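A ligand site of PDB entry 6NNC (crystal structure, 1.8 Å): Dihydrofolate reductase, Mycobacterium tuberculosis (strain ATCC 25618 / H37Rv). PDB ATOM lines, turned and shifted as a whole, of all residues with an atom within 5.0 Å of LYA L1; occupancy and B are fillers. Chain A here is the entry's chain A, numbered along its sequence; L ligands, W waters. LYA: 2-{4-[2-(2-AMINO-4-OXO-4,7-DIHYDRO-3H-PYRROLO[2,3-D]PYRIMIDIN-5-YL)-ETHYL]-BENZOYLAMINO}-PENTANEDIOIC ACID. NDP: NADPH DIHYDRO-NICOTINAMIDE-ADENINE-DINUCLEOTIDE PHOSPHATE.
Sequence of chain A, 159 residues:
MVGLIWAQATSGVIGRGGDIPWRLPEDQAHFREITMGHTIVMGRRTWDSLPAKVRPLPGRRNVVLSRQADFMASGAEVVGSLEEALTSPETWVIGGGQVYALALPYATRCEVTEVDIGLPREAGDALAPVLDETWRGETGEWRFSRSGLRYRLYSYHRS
The side-chain carboxylate of Asp 27 sits at hydrogen-bond distance from the side-chain amide nitrogen of Gln 28 (3.2 Å).
OD1 of Asp 27 is in hydrogen-bond range of OG1 of Thr 113 (2.7 Å).
NE of Arg 60 sits at hydrogen-bond distance from O of Pro 58 (2.9 Å).
The side-chain hydroxyl (OG1) of Thr 35 sits at hydrogen-bond distance from the guanidinium group (NH1) of Arg 60 (2.9 Å).
The backbone carbonyl oxygen (O) of Ile 94 sits close to the side-chain hydroxyl (OH) of Tyr 100 (3.3 Å).
OH of Tyr 100 sits at hydrogen-bond distance from O of Ile 5, at 2.6 Å.
The backbone carbonyl oxygen (O) of Trp 6 is in hydrogen-bond range of the backbone NH (N) of Thr 113, 2.9 Å away.
The backbone carbonyl oxygen of Phe 31 is in hydrogen-bond range of the side-chain hydroxyl of Thr 35 (2.9 Å).
Residues that only touch LYA L1: Ile 94 (3.1 Å), Trp 6 (3.3 Å), Leu 50 (3.4 Å), Phe 31 (3.4 Å), Arg 32 (3.4 Å), Thr 113 (3.6 Å), Ala 7 (3.6 Å), Leu 57 (3.6 Å), Ile 20 (3.9 Å) and Ala 29 (3.9 Å).
Of the 22 residues printed, 15 come within 4 Å of LYA L1.
The nearest printed residue that does not touch LYA L1 is Val 54 (4.1 Å).
Water W2 bridges an oxygen (O28) of LYA L1 (2.7 Å) and the backbone carbonyl oxygen (O) of Pro 25 (2.8 Å).
Water W3 bridges the side-chain amide oxygen of Gln 28 (2.7 Å) and an oxygen (O15) of LYA L1 (2.7 Å).
Water W7 lies within hydrogen-bond range of a nitrogen (N19) of LYA L1, the side-chain hydroxyl (OG1) of Thr 113, a ring nitrogen (NE2) of His 30 and the backbone carbonyl oxygen (O) of Trp 6.
The side-chain carboxylate (OD1) of Asp 27 sits at hydrogen-bond distance from a nitrogen (N19) of LYA L1, at 2.7 Å.
The guanidinium group (NH1) of Arg 60 lies within salt-bridge range of an oxygen (O31) of LYA L1, 2.8 Å away.
NE2 of Gln 28 sits at hydrogen-bond distance from O15 of LYA L1 (2.8 Å).
A nitrogen (N11) of LYA L1 sits at hydrogen-bond distance from the backbone carbonyl oxygen (O) of Ile 5 (3.1 Å).
OH of Tyr 100 is in hydrogen-bond range of N11 of LYA L1 (3.5 Å).
The backbone NH (N) of Ala 7 sits at hydrogen-bond distance from an oxygen (O7N) of NDP L2.
O of Ala 7 is in hydrogen-bond range of N7N of NDP L2, 2.8 Å away.
An oxygen (O1A) of NDP L2 is in hydrogen-bond range of the backbone NH of Thr 46 (3.2 Å).
The side-chain hydroxyl (OG1) of Thr 46 sits at hydrogen-bond distance from an oxygen (O1A) of NDP L2 (2.7 Å).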
ATOM      1  N   ILE A   5      12.640 -28.174 -15.943  1.00  0.00           N
ATOM      2  CA  ILE A   5      11.970 -28.195 -14.649  1.00  0.00           C
ATOM      3  C   ILE A   5      10.902 -29.277 -14.712  1.00  0.00           C
ATOM      4  O   ILE A   5      10.135 -29.341 -15.677  1.00  0.00           O
ATOM      5  CB  ILE A   5      11.395 -26.803 -14.288  1.00  0.00           C
ATOM      6  CG1 ILE A   5      10.703 -26.822 -12.916  1.00  0.00           C
ATOM      7  CG2 ILE A   5      10.429 -26.278 -15.373  1.00  0.00           C
ATOM      8  CD1 ILE A   5      10.362 -25.392 -12.448  1.00  0.00           C
ATOM      9  N   TRP A   6      10.913 -30.173 -13.718  1.00  0.00           N
ATOM     10  CA  TRP A   6       9.944 -31.251 -13.689  1.00  0.00           C
ATOM     11  C   TRP A   6       9.703 -31.699 -12.256  1.00  0.00           C
ATOM     12  O   TRP A   6      10.498 -31.422 -11.342  1.00  0.00           O
ATOM     13  CB  TRP A   6      10.394 -32.456 -14.546  1.00  0.00           C
ATOM     14  CG  TRP A   6      11.478 -33.329 -13.981  1.00  0.00           C
ATOM     15  CD1 TRP A   6      11.339 -34.341 -13.065  1.00  0.00           C
ATOM     16  CD2 TRP A   6      12.870 -33.314 -14.347  1.00  0.00           C
ATOM     17  NE1 TRP A   6      12.567 -34.934 -12.821  1.00  0.00           N
ATOM     18  CE2 TRP A   6      13.520 -34.320 -13.608  1.00  0.00           C
ATOM     19  CE3 TRP A   6      13.636 -32.542 -15.241  1.00  0.00           C
ATOM     20  CZ2 TRP A   6      14.892 -34.578 -13.711  1.00  0.00           C
ATOM     21  CZ3 TRP A   6      14.986 -32.795 -15.353  1.00  0.00           C
ATOM     22  CH2 TRP A   6      15.603 -33.810 -14.592  1.00  0.00           C
ATOM     23  N   ALA A   7       8.592 -32.418 -12.073  1.00  0.00           N
ATOM     24  CA  ALA A   7       8.270 -33.109 -10.826  1.00  0.00           C
ATOM     25  C   ALA A   7       8.194 -34.606 -11.114  1.00  0.00           C
ATOM     26  O   ALA A   7       7.601 -35.020 -12.111  1.00  0.00           O
ATOM     27  CB  ALA A   7       6.955 -32.610 -10.225  1.00  0.00           C
ATOM     28  N   ILE A  20      -0.850 -36.430 -14.883  1.00  0.00           N
ATOM     29  CA  ILE A  20       0.073 -36.594 -13.773  1.00  0.00           C
ATOM     30  C   ILE A  20      -0.683 -37.195 -12.581  1.00  0.00           C
ATOM     31  O   ILE A  20      -1.752 -36.703 -12.245  1.00  0.00           O
ATOM     32  CB  ILE A  20       0.747 -35.272 -13.376  1.00  0.00           C
ATOM     33  CG1 ILE A  20       1.426 -34.615 -14.591  1.00  0.00           C
ATOM     34  CG2 ILE A  20       1.754 -35.458 -12.264  1.00  0.00           C
ATOM     35  CD1 ILE A  20       2.069 -33.271 -14.284  1.00  0.00           C
ATOM     36  N   PRO A  25       0.061 -28.200  -4.764  1.00  0.00           N
ATOM     37  CA  PRO A  25      -0.057 -26.760  -5.042  1.00  0.00           C
ATOM     38  C   PRO A  25       1.256 -26.014  -4.845  1.00  0.00           C
ATOM     39  O   PRO A  25       1.546 -25.082  -5.600  1.00  0.00           O
ATOM     40  CB  PRO A  25      -1.118 -26.293  -4.035  1.00  0.00           C
ATOM     41  CG  PRO A  25      -1.964 -27.514  -3.804  1.00  0.00           C
ATOM     42  CD  PRO A  25      -1.032 -28.694  -3.902  1.00  0.00           C
ATOM     43  N   ASP A  27       4.249 -27.194  -5.411  1.00  0.00           N
ATOM     44  CA  ASP A  27       5.083 -27.445  -6.581  1.00  0.00           C
ATOM     45  C   ASP A  27       4.629 -26.622  -7.778  1.00  0.00           C
ATOM     46  O   ASP A  27       5.467 -26.093  -8.516  1.00  0.00           O
ATOM     47  CB  ASP A  27       5.056 -28.947  -6.905  1.00  0.00           C
ATOM     48  CG  ASP A  27       5.685 -29.265  -8.227  1.00  0.00           C
ATOM     49  OD1 ASP A  27       6.914 -29.130  -8.351  1.00  0.00           O
ATOM     50  OD2 ASP A  27       4.929 -29.625  -9.147  1.00  0.00           O
ATOM     51  N   GLN A  28       3.317 -26.473  -7.968  1.00  0.00           N
ATOM     52  CA  GLN A  28       2.827 -25.605  -9.040  1.00  0.00           C
ATOM     53  C   GLN A  28       3.261 -24.154  -8.823  1.00  0.00           C
ATOM     54  O   GLN A  28       3.619 -23.446  -9.779  1.00  0.00           O
ATOM     55  CB  GLN A  28       1.309 -25.688  -9.138  1.00  0.00           C
ATOM     56  CG  GLN A  28       0.764 -27.102  -9.296  1.00  0.00           C
ATOM     57  CD  GLN A  28       1.191 -27.761 -10.583  1.00  0.00           C
ATOM     58  OE1 GLN A  28       0.455 -27.725 -11.570  1.00  0.00           O
ATOM     59  NE2 GLN A  28       2.351 -28.414 -10.578  1.00  0.00           N
ATOM     60  N   ALA A  29       3.208 -23.673  -7.579  1.00  0.00           N
ATOM     61  CA  ALA A  29       3.655 -22.303  -7.307  1.00  0.00           C
ATOM     62  C   ALA A  29       5.145 -22.155  -7.576  1.00  0.00           C
ATOM     63  O   ALA A  29       5.597 -21.143  -8.124  1.00  0.00           O
ATOM     64  CB  ALA A  29       3.309 -21.915  -5.869  1.00  0.00           C
ATOM     65  N   HIS A  30       5.927 -23.160  -7.181  1.00  0.00           N
ATOM     66  CA  HIS A  30       7.367 -23.173  -7.481  1.00  0.00           C
ATOM     67  C   HIS A  30       7.625 -23.160  -8.984  1.00  0.00           C
ATOM     68  O   HIS A  30       8.503 -22.424  -9.466  1.00  0.00           O
ATOM     69  CB  HIS A  30       7.983 -24.413  -6.818  1.00  0.00           C
ATOM     70  CG  HIS A  30       9.300 -24.838  -7.370  1.00  0.00           C
ATOM     71  ND1 HIS A  30      10.483 -24.183  -7.082  1.00  0.00           N
ATOM     72  CD2 HIS A  30       9.636 -25.906  -8.139  1.00  0.00           C
ATOM     73  CE1 HIS A  30      11.485 -24.807  -7.687  1.00  0.00           C
ATOM     74  NE2 HIS A  30      10.992 -25.856  -8.321  1.00  0.00           N
ATOM     75  N   PHE A  31       6.880 -23.972  -9.734  1.00  0.00           N
ATOM     76  CA  PHE A  31       6.962 -23.942 -11.192  1.00  0.00           C
ATOM     77  C   PHE A  31       6.653 -22.550 -11.723  1.00  0.00           C
ATOM     78  O   PHE A  31       7.368 -22.023 -12.579  1.00  0.00           O
ATOM     79  CB  PHE A  31       6.004 -24.978 -11.797  1.00  0.00           C
ATOM     80  CG  PHE A  31       5.831 -24.863 -13.291  1.00  0.00           C
ATOM     81  CD1 PHE A  31       6.581 -25.647 -14.147  1.00  0.00           C
ATOM     82  CD2 PHE A  31       4.918 -23.947 -13.845  1.00  0.00           C
ATOM     83  CE1 PHE A  31       6.439 -25.539 -15.534  1.00  0.00           C
ATOM     84  CE2 PHE A  31       4.771 -23.833 -15.238  1.00  0.00           C
ATOM     85  CZ  PHE A  31       5.535 -24.642 -16.065  1.00  0.00           C
ATOM     86  N   ARG A  32       5.582 -21.937 -11.207  1.00  0.00           N
ATOM     87  CA  ARG A  32       5.226 -20.603 -11.687  1.00  0.00           C
ATOM     88  C   ARG A  32       6.333 -19.600 -11.409  1.00  0.00           C
ATOM     89  O   ARG A  32       6.664 -18.775 -12.256  1.00  0.00           O
ATOM     90  CB  ARG A  32       3.920 -20.138 -11.063  1.00  0.00           C
ATOM     91  CG  ARG A  32       3.554 -18.710 -11.477  1.00  0.00           C
ATOM     92  CD  ARG A  32       2.240 -18.237 -10.818  1.00  0.00           C
ATOM     93  NE  ARG A  32       2.034 -16.799 -11.014  1.00  0.00           N
ATOM     94  CZ  ARG A  32       2.649 -15.837 -10.326  1.00  0.00           C
ATOM     95  NH1 ARG A  32       3.527 -16.156  -9.388  1.00  0.00           N
ATOM     96  NH2 ARG A  32       2.385 -14.556 -10.576  1.00  0.00           N
ATOM     97  N   THR A  35       9.431 -20.178 -13.842  1.00  0.00           N
ATOM     98  CA  THR A  35       9.252 -19.991 -15.281  1.00  0.00           C
ATOM     99  C   THR A  35       8.714 -18.616 -15.647  1.00  0.00           C
ATOM    100  O   THR A  35       8.891 -18.195 -16.796  1.00  0.00           O
ATOM    101  CB  THR A  35       8.299 -21.053 -15.867  1.00  0.00           C
ATOM    102  OG1 THR A  35       7.024 -20.953 -15.209  1.00  0.00           O
ATOM    103  CG2 THR A  35       8.879 -22.482 -15.679  1.00  0.00           C
ATOM    104  N   THR A  46       2.213 -32.414 -23.867  1.00  0.00           N
ATOM    105  CA  THR A  46       2.106 -31.619 -22.640  1.00  0.00           C
ATOM    106  C   THR A  46       1.229 -30.392 -22.849  1.00  0.00           C
ATOM    107  O   THR A  46       0.443 -30.015 -21.960  1.00  0.00           O
ATOM    108  CB  THR A  46       3.524 -31.270 -22.153  1.00  0.00           C
ATOM    109  OG1 THR A  46       4.173 -32.485 -21.764  1.00  0.00           O
ATOM    110  CG2 THR A  46       3.481 -30.321 -20.955  1.00  0.00           C
ATOM    111  N   SER A  49      -2.168 -31.489 -22.293  1.00  0.00           N
ATOM    112  CA  SER A  49      -2.494 -31.704 -20.886  1.00  0.00           C
ATOM    113  C   SER A  49      -2.930 -30.420 -20.187  1.00  0.00           C
ATOM    114  O   SER A  49      -3.551 -30.475 -19.107  1.00  0.00           O
ATOM    115  CB  SER A  49      -1.307 -32.334 -20.156  1.00  0.00           C
ATOM    116  OG  SER A  49      -0.303 -31.393 -19.814  1.00  0.00           O
ATOM    117  N   LEU A  50      -2.597 -29.262 -20.739  1.00  0.00           N
ATOM    118  CA  LEU A  50      -2.938 -28.002 -20.086  1.00  0.00           C
ATOM    119  C   LEU A  50      -4.443 -27.762 -20.129  1.00  0.00           C
ATOM    120  O   LEU A  50      -5.060 -27.869 -21.198  1.00  0.00           O
ATOM    121  CB  LEU A  50      -2.207 -26.846 -20.754  1.00  0.00           C
ATOM    122  CG  LEU A  50      -0.681 -26.885 -20.696  1.00  0.00           C
ATOM    123  CD1 LEU A  50      -0.106 -25.657 -21.383  1.00  0.00           C
ATOM    124  CD2 LEU A  50      -0.226 -26.958 -19.263  1.00  0.00           C
ATOM    125  N   VAL A  54      -5.539 -22.287 -18.596  1.00  0.00           N
ATOM    126  CA  VAL A  54      -4.159 -21.902 -18.340  1.00  0.00           C
ATOM    127  C   VAL A  54      -3.370 -22.177 -19.620  1.00  0.00           C
ATOM    128  O   VAL A  54      -2.158 -22.428 -19.615  1.00  0.00           O
ATOM    129  CB  VAL A  54      -3.621 -22.645 -17.095  1.00  0.00           C
ATOM    130  CG1 VAL A  54      -3.151 -24.070 -17.394  1.00  0.00           C
ATOM    131  CG2 VAL A  54      -2.606 -21.797 -16.347  1.00  0.00           C
ATOM    132  N   LEU A  57       0.108 -20.526 -20.627  1.00  0.00           N
ATOM    133  CA  LEU A  57       0.486 -20.155 -19.274  1.00  0.00           C
ATOM    134  C   LEU A  57       0.869 -18.683 -19.274  1.00  0.00           C
ATOM    135  O   LEU A  57       1.695 -18.259 -20.104  1.00  0.00           O
ATOM    136  CB  LEU A  57       1.632 -21.049 -18.792  1.00  0.00           C
ATOM    137  CG  LEU A  57       1.275 -22.495 -18.424  1.00  0.00           C
ATOM    138  CD1 LEU A  57       2.503 -23.427 -18.429  1.00  0.00           C
ATOM    139  CD2 LEU A  57       0.617 -22.525 -17.044  1.00  0.00           C
ATOM    140  N   PRO A  58       0.287 -17.871 -18.384  1.00  0.00           N
ATOM    141  CA  PRO A  58       0.388 -16.413 -18.527  1.00  0.00           C
ATOM    142  C   PRO A  58       1.775 -15.857 -18.259  1.00  0.00           C
ATOM    143  O   PRO A  58       2.526 -16.368 -17.422  1.00  0.00           O
ATOM    144  CB  PRO A  58      -0.604 -15.875 -17.487  1.00  0.00           C
ATOM    145  CG  PRO A  58      -1.288 -17.052 -16.888  1.00  0.00           C
ATOM    146  CD  PRO A  58      -0.530 -18.279 -17.235  1.00  0.00           C
ATOM    147  N   ARG A  60       4.362 -15.750 -20.053  1.00  0.00           N
ATOM    148  CA  ARG A  60       5.454 -16.561 -20.584  1.00  0.00           C
ATOM    149  C   ARG A  60       5.261 -16.747 -22.082  1.00  0.00           C
ATOM    150  O   ARG A  60       4.131 -16.791 -22.599  1.00  0.00           O
ATOM    151  CB  ARG A  60       5.509 -17.938 -19.899  1.00  0.00           C
ATOM    152  CG  ARG A  60       6.171 -17.912 -18.534  1.00  0.00           C
ATOM    153  CD  ARG A  60       5.590 -18.994 -17.598  1.00  0.00           C
ATOM    154  NE  ARG A  60       4.272 -18.607 -17.108  1.00  0.00           N
ATOM    155  CZ  ARG A  60       3.621 -19.252 -16.142  1.00  0.00           C
ATOM    156  NH1 ARG A  60       4.185 -20.309 -15.559  1.00  0.00           N
ATOM    157  NH2 ARG A  60       2.433 -18.838 -15.746  1.00  0.00           N
ATOM    158  N   ILE A  94       9.703 -27.559 -20.202  1.00  0.00           N
ATOM    159  CA  ILE A  94       8.760 -28.049 -19.208  1.00  0.00           C
ATOM    160  C   ILE A  94       8.194 -29.412 -19.593  1.00  0.00           C
ATOM    161  O   ILE A  94       7.114 -29.776 -19.154  1.00  0.00           O
ATOM    162  CB  ILE A  94       7.642 -27.010 -18.932  1.00  0.00           C
ATOM    163  CG1 ILE A  94       6.758 -26.805 -20.160  1.00  0.00           C
ATOM    164  CG2 ILE A  94       8.239 -25.683 -18.456  1.00  0.00           C
ATOM    165  CD1 ILE A  94       5.355 -26.182 -19.783  1.00  0.00           C
ATOM    166  N   TYR A 100      12.150 -33.602 -22.668  1.00  0.00           N
ATOM    167  CA  TYR A 100      13.283 -33.525 -21.733  1.00  0.00           C
ATOM    168  C   TYR A 100      14.499 -34.236 -22.303  1.00  0.00           C
ATOM    169  O   TYR A 100      15.631 -33.735 -22.179  1.00  0.00           O
ATOM    170  CB  TYR A 100      12.936 -34.148 -20.365  1.00  0.00           C
ATOM    171  CG  TYR A 100      11.969 -33.354 -19.523  1.00  0.00           C
ATOM    172  CD1 TYR A 100      10.920 -33.990 -18.885  1.00  0.00           C
ATOM    173  CD2 TYR A 100      12.116 -31.985 -19.341  1.00  0.00           C
ATOM    174  CE1 TYR A 100      10.017 -33.294 -18.110  1.00  0.00           C
ATOM    175  CE2 TYR A 100      11.233 -31.265 -18.558  1.00  0.00           C
ATOM    176  CZ  TYR A 100      10.181 -31.931 -17.953  1.00  0.00           C
ATOM    177  OH  TYR A 100       9.252 -31.273 -17.179  1.00  0.00           O
ATOM    178  N   THR A 113      11.457 -31.466  -8.640  1.00  0.00           N
ATOM    179  CA  THR A 113      10.705 -31.753  -7.432  1.00  0.00           C
ATOM    180  C   THR A 113      10.582 -33.263  -7.329  1.00  0.00           C
ATOM    181  O   THR A 113      10.016 -33.904  -8.216  1.00  0.00           O
ATOM    182  CB  THR A 113       9.302 -31.127  -7.451  1.00  0.00           C
ATOM    183  OG1 THR A 113       9.407 -29.720  -7.622  1.00  0.00           O
ATOM    184  CG2 THR A 113       8.612 -31.424  -6.116  1.00  0.00           C
HETATM  185  C1  LYA L   1       2.095 -27.828 -15.902  1.00  0.00           C
HETATM  186  C2  LYA L   1       2.796 -27.026 -14.994  1.00  0.00           C
HETATM  187  C3  LYA L   1       2.109 -25.997 -14.312  1.00  0.00           C
HETATM  188  C4  LYA L   1       0.773 -25.818 -14.571  1.00  0.00           C
HETATM  189  C5  LYA L   1       0.099 -26.596 -15.478  1.00  0.00           C
HETATM  190  C6  LYA L   1       0.750 -27.626 -16.126  1.00  0.00           C
HETATM  191  C7  LYA L   1       2.720 -28.979 -16.685  1.00  0.00           C
HETATM  192  C8  LYA L   1       3.455 -29.987 -15.811  1.00  0.00           C
HETATM  193  C9  LYA L   1       4.882 -29.588 -15.475  1.00  0.00           C
HETATM  194  C10 LYA L   1       5.947 -29.295 -16.345  1.00  0.00           C
HETATM  195  N11 LYA L   1       7.061 -29.031 -15.646  1.00  0.00           N
HETATM  196  C12 LYA L   1       6.775 -29.135 -14.367  1.00  0.00           C
HETATM  197  C13 LYA L   1       5.417 -29.484 -14.185  1.00  0.00           C
HETATM  198  C14 LYA L   1       4.867 -29.653 -12.781  1.00  0.00           C
HETATM  199  O15 LYA L   1       3.733 -29.950 -12.502  1.00  0.00           O
HETATM  200  N16 LYA L   1       5.759 -29.447 -11.735  1.00  0.00           N
HETATM  201  C17 LYA L   1       7.133 -29.083 -11.915  1.00  0.00           C
HETATM  202  N18 LYA L   1       7.660 -28.926 -13.239  1.00  0.00           N
HETATM  203  N19 LYA L   1       7.992 -28.882 -10.771  1.00  0.00           N
HETATM  204  C20 LYA L   1      -0.008 -24.684 -13.913  1.00  0.00           C
HETATM  205  O21 LYA L   1      -1.179 -24.657 -13.765  1.00  0.00           O
HETATM  206  N22 LYA L   1       0.836 -23.570 -13.560  1.00  0.00           N
HETATM  207  C23 LYA L   1       0.382 -22.336 -12.973  1.00  0.00           C
HETATM  208  C24 LYA L   1       0.446 -22.317 -11.472  1.00  0.00           C
HETATM  209  C25 LYA L   1      -0.999 -22.282 -11.015  1.00  0.00           C
HETATM  210  C26 LYA L   1      -1.048 -22.592  -9.534  1.00  0.00           C
HETATM  211  O27 LYA L   1      -1.985 -23.343  -9.102  1.00  0.00           O
HETATM  212  O28 LYA L   1      -0.133 -22.108  -8.804  1.00  0.00           O
HETATM  213  C29 LYA L   1       1.322 -21.258 -13.534  1.00  0.00           C
HETATM  214  O30 LYA L   1       0.900 -20.072 -13.724  1.00  0.00           O
HETATM  215  O31 LYA L   1       2.519 -21.592 -13.756  1.00  0.00           O
HETATM  216  PA  NDP L   2       5.826 -34.817 -24.768  1.00  0.00           P
HETATM  217  O1A NDP L   2       5.123 -33.825 -23.913  1.00  0.00           O
HETATM  218  O2A NDP L   2       7.324 -34.970 -24.671  1.00  0.00           O
HETATM  219  O5B NDP L   2       5.316 -34.413 -26.306  1.00  0.00           O
HETATM  220  C5B NDP L   2       5.648 -35.445 -27.210  1.00  0.00           C
HETATM  221  C4B NDP L   2       5.355 -34.788 -28.592  1.00  0.00           C
HETATM  222  O4B NDP L   2       6.256 -33.703 -28.799  1.00  0.00           O
HETATM  223  C3B NDP L   2       5.485 -35.751 -29.801  1.00  0.00           C
HETATM  224  O3B NDP L   2       4.268 -36.487 -29.953  1.00  0.00           O
HETATM  225  C2B NDP L   2       5.627 -34.686 -30.947  1.00  0.00           C
HETATM  226  O2B NDP L   2       4.520 -33.996 -31.160  1.00  0.00           O
HETATM  227  C1B NDP L   2       6.590 -33.680 -30.219  1.00  0.00           C
HETATM  228  N9A NDP L   2       8.009 -34.017 -30.422  1.00  0.00           N
HETATM  229  C8A NDP L   2       8.836 -34.935 -29.770  1.00  0.00           C
HETATM  230  N7A NDP L   2      10.102 -34.986 -30.273  1.00  0.00           N
HETATM  231  C5A NDP L   2      10.080 -34.036 -31.322  1.00  0.00           C
HETATM  232  C6A NDP L   2      11.057 -33.589 -32.236  1.00  0.00           C
HETATM  233  N6A NDP L   2      12.350 -34.077 -32.257  1.00  0.00           N
HETATM  234  N1A NDP L   2      10.743 -32.629 -33.172  1.00  0.00           N
HETATM  235  C2A NDP L   2       9.450 -32.163 -33.139  1.00  0.00           C
HETATM  236  N3A NDP L   2       8.425 -32.490 -32.330  1.00  0.00           N
HETATM  237  C4A NDP L   2       8.772 -33.442 -31.416  1.00  0.00           C
HETATM  238  O3  NDP L   2       5.029 -36.277 -24.553  1.00  0.00           O
HETATM  239  PN  NDP L   2       5.414 -37.276 -23.349  1.00  0.00           P
HETATM  240  O1N NDP L   2       4.362 -38.310 -23.481  1.00  0.00           O
HETATM  241  O2N NDP L   2       6.859 -37.708 -23.218  1.00  0.00           O
HETATM  242  O5D NDP L   2       5.117 -36.499 -21.887  1.00  0.00           O
HETATM  243  C5D NDP L   2       3.749 -36.181 -21.718  1.00  0.00           C
HETATM  244  C4D NDP L   2       3.372 -36.706 -20.334  1.00  0.00           C
HETATM  245  O4D NDP L   2       4.280 -36.166 -19.315  1.00  0.00           O
HETATM  246  C3D NDP L   2       1.913 -36.319 -19.907  1.00  0.00           C
HETATM  247  O3D NDP L   2       1.493 -37.363 -19.047  1.00  0.00           O
HETATM  248  C2D NDP L   2       2.143 -35.055 -19.094  1.00  0.00           C
HETATM  249  O2D NDP L   2       1.123 -34.835 -18.125  1.00  0.00           O
HETATM  250  C1D NDP L   2       3.480 -35.460 -18.356  1.00  0.00           C
HETATM  251  N1N NDP L   2       4.258 -34.296 -17.881  1.00  0.00           N
HETATM  252  C2N NDP L   2       4.694 -34.270 -16.568  1.00  0.00           C
HETATM  253  C3N NDP L   2       5.596 -33.341 -16.160  1.00  0.00           C
HETATM  254  C7N NDP L   2       6.100 -33.350 -14.790  1.00  0.00           C
HETATM  255  O7N NDP L   2       6.960 -32.552 -14.404  1.00  0.00           O
HETATM  256  N7N NDP L   2       5.613 -34.262 -13.894  1.00  0.00           N
HETATM  257  C4N NDP L   2       6.129 -32.298 -17.076  1.00  0.00           C
HETATM  258  C5N NDP L   2       5.520 -32.347 -18.429  1.00  0.00           C
HETATM  259  C6N NDP L   2       4.650 -33.286 -18.788  1.00  0.00           C
HETATM  260  P2B NDP L   2       3.423 -34.458 -32.468  1.00  0.00           P
HETATM  261  O1X NDP L   2       3.006 -35.810 -31.970  1.00  0.00           O
HETATM  262  O2X NDP L   2       2.348 -33.355 -32.394  1.00  0.00           O
HETATM  263  O3X NDP L   2       4.359 -34.403 -33.635  1.00  0.00           O
HETATM  264  O   HOH W   1      -2.840 -24.099  -6.402  1.00  0.00           O
HETATM  265  O   HOH W   2      -0.236 -23.089  -6.257  1.00  0.00           O
HETATM  266  O   HOH W   3       1.090 -29.740 -13.202  1.00  0.00           O
HETATM  267  O   HOH W   4      -3.474 -26.103 -10.438  1.00  0.00           O
HETATM  268  O   HOH W   5      -0.082 -30.880 -15.517  1.00  0.00           O
HETATM  269  O   HOH W   6      -1.449 -19.131 -13.296  1.00  0.00           O
HETATM  270  O   HOH W   7      10.701 -28.419  -9.914  1.00  0.00           O
